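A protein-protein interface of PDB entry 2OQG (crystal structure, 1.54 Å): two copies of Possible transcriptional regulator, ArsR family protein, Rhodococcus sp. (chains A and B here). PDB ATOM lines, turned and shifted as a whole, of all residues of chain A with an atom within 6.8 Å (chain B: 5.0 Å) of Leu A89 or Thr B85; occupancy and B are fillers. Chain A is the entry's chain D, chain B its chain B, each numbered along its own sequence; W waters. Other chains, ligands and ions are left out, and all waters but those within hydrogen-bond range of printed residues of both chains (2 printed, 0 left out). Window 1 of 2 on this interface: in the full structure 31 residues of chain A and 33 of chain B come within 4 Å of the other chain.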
ATOM      1  N   LEU A  11     -26.624 -13.421  27.096  1.00  0.00           N
ATOM      2  CA  LEU A  11     -25.905 -14.272  26.110  1.00  0.00           C
ATOM      3  C   LEU A  11     -26.820 -15.319  25.506  1.00  0.00           C
ATOM      4  O   LEU A  11     -26.894 -15.451  24.264  1.00  0.00           O
ATOM      5  CB  LEU A  11     -24.657 -14.939  26.712  1.00  0.00           C
ATOM      6  CG  LEU A  11     -23.440 -14.065  26.862  1.00  0.00           C
ATOM      7  CD1 LEU A  11     -22.414 -14.831  27.755  1.00  0.00           C
ATOM      8  CD2 LEU A  11     -22.863 -13.685  25.519  1.00  0.00           C
ATOM      9  N   PHE A  15     -27.805 -15.765  21.537  1.00  0.00           N
ATOM     10  CA  PHE A  15     -27.598 -17.011  20.788  1.00  0.00           C
ATOM     11  C   PHE A  15     -28.894 -17.731  20.370  1.00  0.00           C
ATOM     12  O   PHE A  15     -28.950 -18.281  19.258  1.00  0.00           O
ATOM     13  CB  PHE A  15     -26.572 -17.871  21.511  1.00  0.00           C
ATOM     14  CG  PHE A  15     -25.202 -17.313  21.376  1.00  0.00           C
ATOM     15  CD1 PHE A  15     -24.579 -17.288  20.102  1.00  0.00           C
ATOM     16  CD2 PHE A  15     -24.583 -16.667  22.454  1.00  0.00           C
ATOM     17  CE1 PHE A  15     -23.309 -16.703  19.936  1.00  0.00           C
ATOM     18  CE2 PHE A  15     -23.319 -16.106  22.306  1.00  0.00           C
ATOM     19  CZ  PHE A  15     -22.690 -16.117  21.047  1.00  0.00           C
ATOM     20  N   LEU A  18     -29.814 -15.957  17.227  1.00  0.00           N
ATOM     21  CA  LEU A  18     -28.915 -16.245  16.096  1.00  0.00           C
ATOM     22  C   LEU A  18     -29.062 -17.668  15.609  1.00  0.00           C
ATOM     23  O   LEU A  18     -28.622 -18.002  14.473  1.00  0.00           O
ATOM     24  CB  LEU A  18     -27.459 -16.023  16.499  1.00  0.00           C
ATOM     25  CG  LEU A  18     -26.973 -14.606  16.859  1.00  0.00           C
ATOM     26  CD1 LEU A  18     -25.490 -14.602  17.239  1.00  0.00           C
ATOM     27  CD2 LEU A  18     -27.210 -13.630  15.707  1.00  0.00           C
ATOM     28  N   LYS A  84     -20.601  -6.401  22.087  1.00  0.00           N
ATOM     29  CA  LYS A  84     -20.695  -6.705  23.513  1.00  0.00           C
ATOM     30  C   LYS A  84     -20.628  -8.243  23.722  1.00  0.00           C
ATOM     31  O   LYS A  84     -19.965  -8.742  24.649  1.00  0.00           O
ATOM     32  CB  LYS A  84     -22.005  -6.166  24.068  1.00  0.00           C
ATOM     33  CG  LYS A  84     -22.093  -6.155  25.590  1.00  0.00           C
ATOM     34  CD  LYS A  84     -23.466  -5.673  26.067  1.00  0.00           C
ATOM     35  CE  LYS A  84     -23.686  -5.844  27.582  1.00  0.00           C
ATOM     36  NZ  LYS A  84     -23.416  -7.217  28.118  1.00  0.00           N
ATOM     37  N   THR A  85     -21.329  -8.970  22.857  1.00  0.00           N
ATOM     38  CA  THR A  85     -21.350 -10.437  22.900  1.00  0.00           C
ATOM     39  C   THR A  85     -19.943 -10.984  22.616  1.00  0.00           C
ATOM     40  O   THR A  85     -19.440 -11.844  23.377  1.00  0.00           O
ATOM     41  CB  THR A  85     -22.398 -11.001  21.921  1.00  0.00           C
ATOM     42  OG1 THR A  85     -23.686 -10.482  22.283  1.00  0.00           O
ATOM     43  CG2 THR A  85     -22.432 -12.565  21.941  1.00  0.00           C
ATOM     44  N   ALA A  86     -19.301 -10.446  21.579  1.00  0.00           N
ATOM     45  CA  ALA A  86     -17.964 -10.884  21.138  1.00  0.00           C
ATOM     46  C   ALA A  86     -16.949 -10.629  22.225  1.00  0.00           C
ATOM     47  O   ALA A  86     -16.067 -11.474  22.487  1.00  0.00           O
ATOM     48  CB  ALA A  86     -17.557 -10.147  19.887  1.00  0.00           C
ATOM     49  N   ARG A  87     -17.080  -9.477  22.872  1.00  0.00           N
ATOM     50  CA  ARG A  87     -16.153  -9.109  23.929  1.00  0.00           C
ATOM     51  C   ARG A  87     -16.316  -9.986  25.153  1.00  0.00           C
ATOM     52  O   ARG A  87     -15.320 -10.341  25.781  1.00  0.00           O
ATOM     53  CB  ARG A  87     -16.250  -7.628  24.319  1.00  0.00           C
ATOM     54  CG  ARG A  87     -15.443  -6.714  23.390  1.00  0.00           C
ATOM     55  CD  ARG A  87     -15.926  -5.276  23.459  1.00  0.00           C
ATOM     56  NE  ARG A  87     -15.096  -4.409  22.618  1.00  0.00           N
ATOM     57  CZ  ARG A  87     -13.958  -3.828  23.018  1.00  0.00           C
ATOM     58  NH1 ARG A  87     -13.518  -3.995  24.265  1.00  0.00           N
ATOM     59  NH2 ARG A  87     -13.266  -3.064  22.174  1.00  0.00           N
ATOM     60  N   THR A  88     -17.552 -10.331  25.504  1.00  0.00           N
ATOM     61  CA  THR A  88     -17.816 -11.267  26.602  1.00  0.00           C
ATOM     62  C   THR A  88     -17.250 -12.671  26.277  1.00  0.00           C
ATOM     63  O   THR A  88     -16.614 -13.309  27.122  1.00  0.00           O
ATOM     64  CB  THR A  88     -19.308 -11.379  26.857  1.00  0.00           C
ATOM     65  OG1 THR A  88     -19.814 -10.107  27.295  1.00  0.00           O
ATOM     66  CG2 THR A  88     -19.607 -12.400  27.917  1.00  0.00           C
ATOM     67  N   LEU A  89     -17.464 -13.148  25.054  1.00  0.00           N
ATOM     68  CA  LEU A  89     -16.913 -14.473  24.705  1.00  0.00           C
ATOM     69  C   LEU A  89     -15.374 -14.483  24.746  1.00  0.00           C
ATOM     70  O   LEU A  89     -14.758 -15.479  25.095  1.00  0.00           O
ATOM     71  CB  LEU A  89     -17.427 -14.955  23.350  1.00  0.00           C
ATOM     72  CG  LEU A  89     -18.709 -15.816  23.363  1.00  0.00           C
ATOM     73  CD1 LEU A  89     -19.858 -15.136  24.058  1.00  0.00           C
ATOM     74  CD2 LEU A  89     -19.117 -16.283  21.980  1.00  0.00           C
ATOM     75  N   GLU A  90     -14.776 -13.373  24.350  1.00  0.00           N
ATOM     76  CA  GLU A  90     -13.330 -13.273  24.314  1.00  0.00           C
ATOM     77  C   GLU A  90     -12.733 -13.278  25.714  1.00  0.00           C
ATOM     78  O   GLU A  90     -11.692 -13.880  25.928  1.00  0.00           O
ATOM     79  CB  GLU A  90     -12.891 -12.059  23.476  1.00  0.00           C
ATOM     80  CG  GLU A  90     -12.815 -12.419  21.998  1.00  0.00           C
ATOM     81  CD  GLU A  90     -12.873 -11.238  21.027  1.00  0.00           C
ATOM     82  OE1 GLU A  90     -13.617 -10.272  21.278  1.00  0.00           O
ATOM     83  OE2 GLU A  90     -12.191 -11.302  19.976  1.00  0.00           O
ATOM     84  N   ARG A  91     -13.404 -12.648  26.674  1.00  0.00           N
ATOM     85  CA  ARG A  91     -12.947 -12.682  28.044  1.00  0.00           C
ATOM     86  C   ARG A  91     -13.038 -14.107  28.582  1.00  0.00           C
ATOM     87  O   ARG A  91     -12.044 -14.652  29.100  1.00  0.00           O
ATOM     88  CB  ARG A  91     -13.768 -11.761  28.946  1.00  0.00           C
ATOM     89  CG  ARG A  91     -13.180 -11.666  30.347  1.00  0.00           C
ATOM     90  CD  ARG A  91     -14.194 -11.252  31.395  1.00  0.00           C
ATOM     91  NE  ARG A  91     -15.133 -12.321  31.730  1.00  0.00           N
ATOM     92  CZ  ARG A  91     -16.458 -12.213  31.630  1.00  0.00           C
ATOM     93  NH1 ARG A  91     -17.237 -13.238  31.966  1.00  0.00           N
ATOM     94  NH2 ARG A  91     -17.013 -11.078  31.207  1.00  0.00           N
ATOM     95  N   ILE A  92     -14.230 -14.698  28.465  1.00  0.00           N
ATOM     96  CA  ILE A  92     -14.456 -16.082  28.927  1.00  0.00           C
ATOM     97  C   ILE A  92     -13.486 -17.069  28.266  1.00  0.00           C
ATOM     98  O   ILE A  92     -12.865 -17.891  28.935  1.00  0.00           O
ATOM     99  CB  ILE A  92     -15.913 -16.537  28.663  1.00  0.00           C
ATOM    100  CG1 ILE A  92     -16.895 -15.593  29.349  1.00  0.00           C
ATOM    101  CG2 ILE A  92     -16.148 -17.986  29.127  1.00  0.00           C
ATOM    102  CD1 ILE A  92     -18.322 -15.793  28.860  1.00  0.00           C
ATOM    103  N   GLY A  93     -13.357 -16.974  26.954  1.00  0.00           N
ATOM    104  CA  GLY A  93     -12.464 -17.819  26.203  1.00  0.00           C
ATOM    105  C   GLY A  93     -11.059 -17.706  26.744  1.00  0.00           C
ATOM    106  O   GLY A  93     -10.413 -18.734  27.003  1.00  0.00           O
ATOM    107  N   ALA A  94     -10.598 -16.468  26.952  1.00  0.00           N
ATOM    108  CA  ALA A  94      -9.259 -16.211  27.521  1.00  0.00           C
ATOM    109  C   ALA A  94      -9.040 -16.908  28.864  1.00  0.00           C
ATOM    110  O   ALA A  94      -7.957 -17.420  29.117  1.00  0.00           O
ATOM    111  CB  ALA A  94      -9.031 -14.693  27.685  1.00  0.00           C
ATOM    112  N   GLU A  95     -10.061 -16.916  29.718  1.00  0.00           N
ATOM    113  CA  GLU A  95      -9.950 -17.523  31.049  1.00  0.00           C
ATOM    114  C   GLU A  95      -9.888 -19.056  30.982  1.00  0.00           C
ATOM    115  O   GLU A  95      -9.245 -19.689  31.817  1.00  0.00           O
ATOM    116  CB  GLU A  95     -11.122 -17.117  31.940  1.00  0.00           C
ATOM    117  CG  GLU A  95     -11.309 -15.628  32.118  1.00  0.00           C
ATOM    118  CD  GLU A  95     -12.754 -15.268  32.410  1.00  0.00           C
ATOM    119  OE1 GLU A  95     -13.543 -16.167  32.805  1.00  0.00           O
ATOM    120  OE2 GLU A  95     -13.110 -14.082  32.243  1.00  0.00           O
ATOM    121  N   LEU B  11     -21.614 -22.447  12.168  1.00  0.00           N
ATOM    122  CA  LEU B  11     -21.786 -22.001  13.561  1.00  0.00           C
ATOM    123  C   LEU B  11     -23.141 -22.421  14.205  1.00  0.00           C
ATOM    124  O   LEU B  11     -23.329 -22.259  15.425  1.00  0.00           O
ATOM    125  CB  LEU B  11     -21.572 -20.501  13.683  1.00  0.00           C
ATOM    126  CG  LEU B  11     -20.144 -20.021  13.353  1.00  0.00           C
ATOM    127  CD1 LEU B  11     -20.054 -18.572  13.783  1.00  0.00           C
ATOM    128  CD2 LEU B  11     -19.075 -20.851  14.092  1.00  0.00           C
ATOM    129  N   VAL B  14     -23.071 -24.495  17.456  1.00  0.00           N
ATOM    130  CA  VAL B  14     -22.580 -23.666  18.535  1.00  0.00           C
ATOM    131  C   VAL B  14     -23.631 -22.667  19.015  1.00  0.00           C
ATOM    132  O   VAL B  14     -23.865 -22.560  20.211  1.00  0.00           O
ATOM    133  CB  VAL B  14     -21.249 -22.981  18.170  1.00  0.00           C
ATOM    134  CG1 VAL B  14     -20.874 -21.925  19.196  1.00  0.00           C
ATOM    135  CG2 VAL B  14     -20.168 -24.047  18.145  1.00  0.00           C
ATOM    136  N   PHE B  15     -24.264 -21.946  18.099  1.00  0.00           N
ATOM    137  CA  PHE B  15     -25.309 -21.008  18.506  1.00  0.00           C
ATOM    138  C   PHE B  15     -26.378 -21.761  19.295  1.00  0.00           C
ATOM    139  O   PHE B  15     -26.808 -21.275  20.308  1.00  0.00           O
ATOM    140  CB  PHE B  15     -25.974 -20.330  17.283  1.00  0.00           C
ATOM    141  CG  PHE B  15     -25.064 -19.440  16.476  1.00  0.00           C
ATOM    142  CD1 PHE B  15     -23.884 -18.928  17.007  1.00  0.00           C
ATOM    143  CD2 PHE B  15     -25.449 -19.069  15.174  1.00  0.00           C
ATOM    144  CE1 PHE B  15     -23.091 -18.040  16.227  1.00  0.00           C
ATOM    145  CE2 PHE B  15     -24.636 -18.231  14.411  1.00  0.00           C
ATOM    146  CZ  PHE B  15     -23.476 -17.744  14.942  1.00  0.00           C
ATOM    147  N   LEU B  18     -25.215 -22.543  22.782  1.00  0.00           N
ATOM    148  CA  LEU B  18     -25.103 -21.346  23.619  1.00  0.00           C
ATOM    149  C   LEU B  18     -26.453 -20.658  23.855  1.00  0.00           C
ATOM    150  O   LEU B  18     -26.511 -19.632  24.502  1.00  0.00           O
ATOM    151  CB  LEU B  18     -24.050 -20.353  23.028  1.00  0.00           C
ATOM    152  CG  LEU B  18     -22.616 -20.870  22.880  1.00  0.00           C
ATOM    153  CD1 LEU B  18     -21.679 -19.817  22.266  1.00  0.00           C
ATOM    154  CD2 LEU B  18     -22.053 -21.399  24.207  1.00  0.00           C
ATOM    155  N   TRP B  24     -24.745 -22.543  29.776  1.00  0.00           N
ATOM    156  CA  TRP B  24     -23.761 -21.544  30.205  1.00  0.00           C
ATOM    157  C   TRP B  24     -23.244 -21.796  31.620  1.00  0.00           C
ATOM    158  O   TRP B  24     -22.036 -21.614  31.894  1.00  0.00           O
ATOM    159  CB  TRP B  24     -24.303 -20.112  30.072  1.00  0.00           C
ATOM    160  CG  TRP B  24     -24.160 -19.573  28.675  1.00  0.00           C
ATOM    161  CD1 TRP B  24     -25.155 -19.443  27.730  1.00  0.00           C
ATOM    162  CD2 TRP B  24     -22.941 -19.120  28.049  1.00  0.00           C
ATOM    163  NE1 TRP B  24     -24.621 -18.943  26.552  1.00  0.00           N
ATOM    164  CE2 TRP B  24     -23.273 -18.717  26.728  1.00  0.00           C
ATOM    165  CE3 TRP B  24     -21.604 -19.034  28.477  1.00  0.00           C
ATOM    166  CZ2 TRP B  24     -22.308 -18.205  25.831  1.00  0.00           C
ATOM    167  CZ3 TRP B  24     -20.635 -18.562  27.580  1.00  0.00           C
ATOM    168  CH2 TRP B  24     -21.004 -18.123  26.289  1.00  0.00           C
ATOM    169  N   GLU B  81     -13.971 -22.738  20.336  1.00  0.00           N
ATOM    170  CA  GLU B  81     -15.191 -22.353  19.582  1.00  0.00           C
ATOM    171  C   GLU B  81     -15.715 -21.008  20.041  1.00  0.00           C
ATOM    172  O   GLU B  81     -16.328 -20.299  19.227  1.00  0.00           O
ATOM    173  CB  GLU B  81     -16.318 -23.405  19.687  1.00  0.00           C
ATOM    174  CG  GLU B  81     -15.960 -24.773  19.168  1.00  0.00           C
ATOM    175  CD  GLU B  81     -15.801 -24.800  17.672  1.00  0.00           C
ATOM    176  OE1 GLU B  81     -16.248 -23.841  16.987  1.00  0.00           O
ATOM    177  OE2 GLU B  81     -15.207 -25.778  17.179  1.00  0.00           O
ATOM    178  N   LEU B  82     -15.461 -20.622  21.304  1.00  0.00           N
ATOM    179  CA  LEU B  82     -15.866 -19.294  21.778  1.00  0.00           C
ATOM    180  C   LEU B  82     -15.064 -18.235  21.035  1.00  0.00           C
ATOM    181  O   LEU B  82     -15.615 -17.241  20.588  1.00  0.00           O
ATOM    182  CB  LEU B  82     -15.716 -19.117  23.301  1.00  0.00           C
ATOM    183  CG  LEU B  82     -16.696 -19.786  24.275  1.00  0.00           C
ATOM    184  CD1 LEU B  82     -16.542 -18.995  25.598  1.00  0.00           C
ATOM    185  CD2 LEU B  82     -18.138 -19.775  23.769  1.00  0.00           C
ATOM    186  N   ASN B  83     -13.757 -18.459  20.918  1.00  0.00           N
ATOM    187  CA  ASN B  83     -12.860 -17.564  20.181  1.00  0.00           C
ATOM    188  C   ASN B  83     -13.239 -17.482  18.684  1.00  0.00           C
ATOM    189  O   ASN B  83     -13.292 -16.375  18.111  1.00  0.00           O
ATOM    190  CB  ASN B  83     -11.391 -17.976  20.406  1.00  0.00           C
ATOM    191  CG  ASN B  83     -10.993 -17.952  21.896  1.00  0.00           C
ATOM    192  OD1 ASN B  83     -11.612 -17.263  22.716  1.00  0.00           O
ATOM    193  ND2 ASN B  83      -9.961 -18.707  22.247  1.00  0.00           N
ATOM    194  N   LYS B  84     -13.504 -18.609  18.042  1.00  0.00           N
ATOM    195  CA  LYS B  84     -13.910 -18.575  16.637  1.00  0.00           C
ATOM    196  C   LYS B  84     -15.223 -17.802  16.445  1.00  0.00           C
ATOM    197  O   LYS B  84     -15.422 -17.037  15.476  1.00  0.00           O
ATOM    198  CB  LYS B  84     -14.073 -20.003  16.098  1.00  0.00           C
ATOM    199  CG  LYS B  84     -14.564 -20.066  14.659  1.00  0.00           C
ATOM    200  CD  LYS B  84     -14.934 -21.481  14.260  1.00  0.00           C
ATOM    201  CE  LYS B  84     -13.829 -22.168  13.500  1.00  0.00           C
ATOM    202  NZ  LYS B  84     -14.336 -23.421  12.909  1.00  0.00           N
ATOM    203  N   THR B  85     -16.163 -18.027  17.366  1.00  0.00           N
ATOM    204  CA  THR B  85     -17.456 -17.342  17.284  1.00  0.00           C
ATOM    205  C   THR B  85     -17.279 -15.832  17.490  1.00  0.00           C
ATOM    206  O   THR B  85     -17.876 -15.031  16.773  1.00  0.00           O
ATOM    207  CB  THR B  85     -18.469 -17.926  18.313  1.00  0.00           C
ATOM    208  OG1 THR B  85     -18.618 -19.325  18.080  1.00  0.00           O
ATOM    209  CG2 THR B  85     -19.834 -17.255  18.195  1.00  0.00           C
ATOM    210  N   ALA B  86     -16.451 -15.468  18.460  1.00  0.00           N
ATOM    211  CA  ALA B  86     -16.177 -14.086  18.808  1.00  0.00           C
ATOM    212  C   ALA B  86     -15.523 -13.412  17.634  1.00  0.00           C
ATOM    213  O   ALA B  86     -15.905 -12.288  17.335  1.00  0.00           O
ATOM    214  CB  ALA B  86     -15.272 -14.000  20.012  1.00  0.00           C
ATOM    215  N   ARG B  87     -14.595 -14.098  16.948  1.00  0.00           N
ATOM    216  CA  ARG B  87     -13.916 -13.531  15.747  1.00  0.00           C
ATOM    217  C   ARG B  87     -14.961 -13.170  14.688  1.00  0.00           C
ATOM    218  O   ARG B  87     -14.922 -12.072  14.111  1.00  0.00           O
ATOM    219  CB  ARG B  87     -12.856 -14.495  15.139  1.00  0.00           C
ATOM    220  CG  ARG B  87     -11.506 -14.508  15.863  1.00  0.00           C
ATOM    221  CD  ARG B  87     -10.371 -15.272  15.121  1.00  0.00           C
ATOM    222  NE  ARG B  87     -10.732 -16.611  14.637  1.00  0.00           N
ATOM    223  CZ  ARG B  87     -10.503 -17.737  15.318  1.00  0.00           C
ATOM    224  NH1 ARG B  87      -9.935 -17.683  16.533  1.00  0.00           N
ATOM    225  NH2 ARG B  87     -10.882 -18.911  14.819  1.00  0.00           N
ATOM    226  N   THR B  88     -15.877 -14.107  14.434  1.00  0.00           N
ATOM    227  CA  THR B  88     -16.929 -13.940  13.444  1.00  0.00           C
ATOM    228  C   THR B  88     -17.909 -12.825  13.828  1.00  0.00           C
ATOM    229  O   THR B  88     -18.269 -11.989  12.978  1.00  0.00           O
ATOM    230  CB  THR B  88     -17.696 -15.253  13.232  1.00  0.00           C
ATOM    231  OG1 THR B  88     -16.775 -16.298  12.888  1.00  0.00           O
ATOM    232  CG2 THR B  88     -18.727 -15.107  12.177  1.00  0.00           C
ATOM    233  N   LEU B  89     -18.335 -12.780  15.089  1.00  0.00           N
ATOM    234  CA  LEU B  89     -19.256 -11.708  15.515  1.00  0.00           C
ATOM    235  C   LEU B  89     -18.612 -10.326  15.472  1.00  0.00           C
ATOM    236  O   LEU B  89     -19.261  -9.339  15.158  1.00  0.00           O
ATOM    237  CB  LEU B  89     -19.825 -11.962  16.892  1.00  0.00           C
ATOM    238  CG  LEU B  89     -20.567 -13.298  16.973  1.00  0.00           C
ATOM    239  CD1 LEU B  89     -21.171 -13.429  18.347  1.00  0.00           C
ATOM    240  CD2 LEU B  89     -21.626 -13.511  15.849  1.00  0.00           C
ATOM    241  N   GLU B  90     -17.328 -10.265  15.782  1.00  0.00           N
ATOM    242  CA  GLU B  90     -16.606  -9.023  15.782  1.00  0.00           C
ATOM    243  C   GLU B  90     -16.503  -8.451  14.369  1.00  0.00           C
ATOM    244  O   GLU B  90     -16.708  -7.236  14.153  1.00  0.00           O
ATOM    245  CB  GLU B  90     -15.221  -9.281  16.339  1.00  0.00           C
ATOM    246  CG  GLU B  90     -14.683  -8.119  17.092  1.00  0.00           C
ATOM    247  CD  GLU B  90     -13.574  -8.546  18.028  1.00  0.00           C
ATOM    248  OE1 GLU B  90     -13.890  -9.172  19.070  1.00  0.00           O
ATOM    249  OE2 GLU B  90     -12.393  -8.260  17.719  1.00  0.00           O
HETATM  250  O   HOH W   1     -11.708 -14.571  19.186  1.00  0.00           O
HETATM  251  O   HOH W   2     -10.227 -14.692  23.981  1.00  0.00           O
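Phe A15 touches Phe B15.
Leu B18 touches Phe A15.
Phe A15 touches Thr B85.
Leu A18 touches Phe B15 (O to CD2, 3.4 Å).
CG2 of Thr A85 touches CD1 of Leu B89 (3.9 Å).
Ala B86 touches Ala A86.
CH2 of Trp B24 touches CD1 of Leu A89, 3.9 Å away.
Leu A89 touches Leu B82.
CB of Ala B86 touches CG of Glu A90, 3.5 Å away.
Leu B82 touches Ile A92.
OE1 of Glu B90 sits close to OE1 of Glu A90 (2.5 Å).
Of the printed residues of chain B, Leu A11 touches Trp B24.
Of the printed residues of chain B, Ala A86 touches Ala B86 and Glu B90.
Arg A87 touches none of the printed residues of chain B.
Of chain B, only Trp B24 (3.9 Å), Leu B82 (3.9 Å) and Thr B85 (3.97 Å) come within 4 Å of Leu A89.
Ala A94 touches none of the printed residues of chain B.
Of chain A, only Phe A15 (3.9 Å) and Leu A89 (3.97 Å) come within 4 Å of Thr B85.
The nearest residue of chain B that does not touch Leu A89 is Ala B86 (4.1 Å).
Of the 15 printed residues of chain A, 9 touch a printed residue of chain B.
Hydrophobic or aromatic side chains of chain A that line the printed part of chain B: Leu A11, Phe A15, Leu A18, Ala A86, Leu A89 and Ile A92.
Phe A15 touches its own counterpart, Phe B15.
Phe A15 touches Leu B18, and with the chains exchanged Leu A18 touches Phe B15.
Ala A86 touches Glu B90, and with the chains exchanged Glu A90 touches Ala B86.
Glu A90 touches its own counterpart, Glu B90.
Of the 16 pairs that touch across the chains among the printed residues, 9 have their exchanged pair printed and touching as well.
Water W2 lies within hydrogen-bond range of the backbone carbonyl oxygen (O) of Glu A90, the side-chain amide oxygen (OD1) of Asn B83 and the backbone NH (N) of Ala A94.
Water W1 lies within hydrogen-bond range of O of Asn B83 (2.6 Å) and OE2 of Glu A90 (3.4 Å).
The backbone carbonyl oxygen (O) of Glu B81 lies within hydrogen-bond range of the side-chain hydroxyl (OG1) of Thr B85, at 2.7 Å.
The backbone carbonyl oxygen of Leu B18 sits at hydrogen-bond distance from the indole nitrogen of Trp B24 (2.9 Å).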
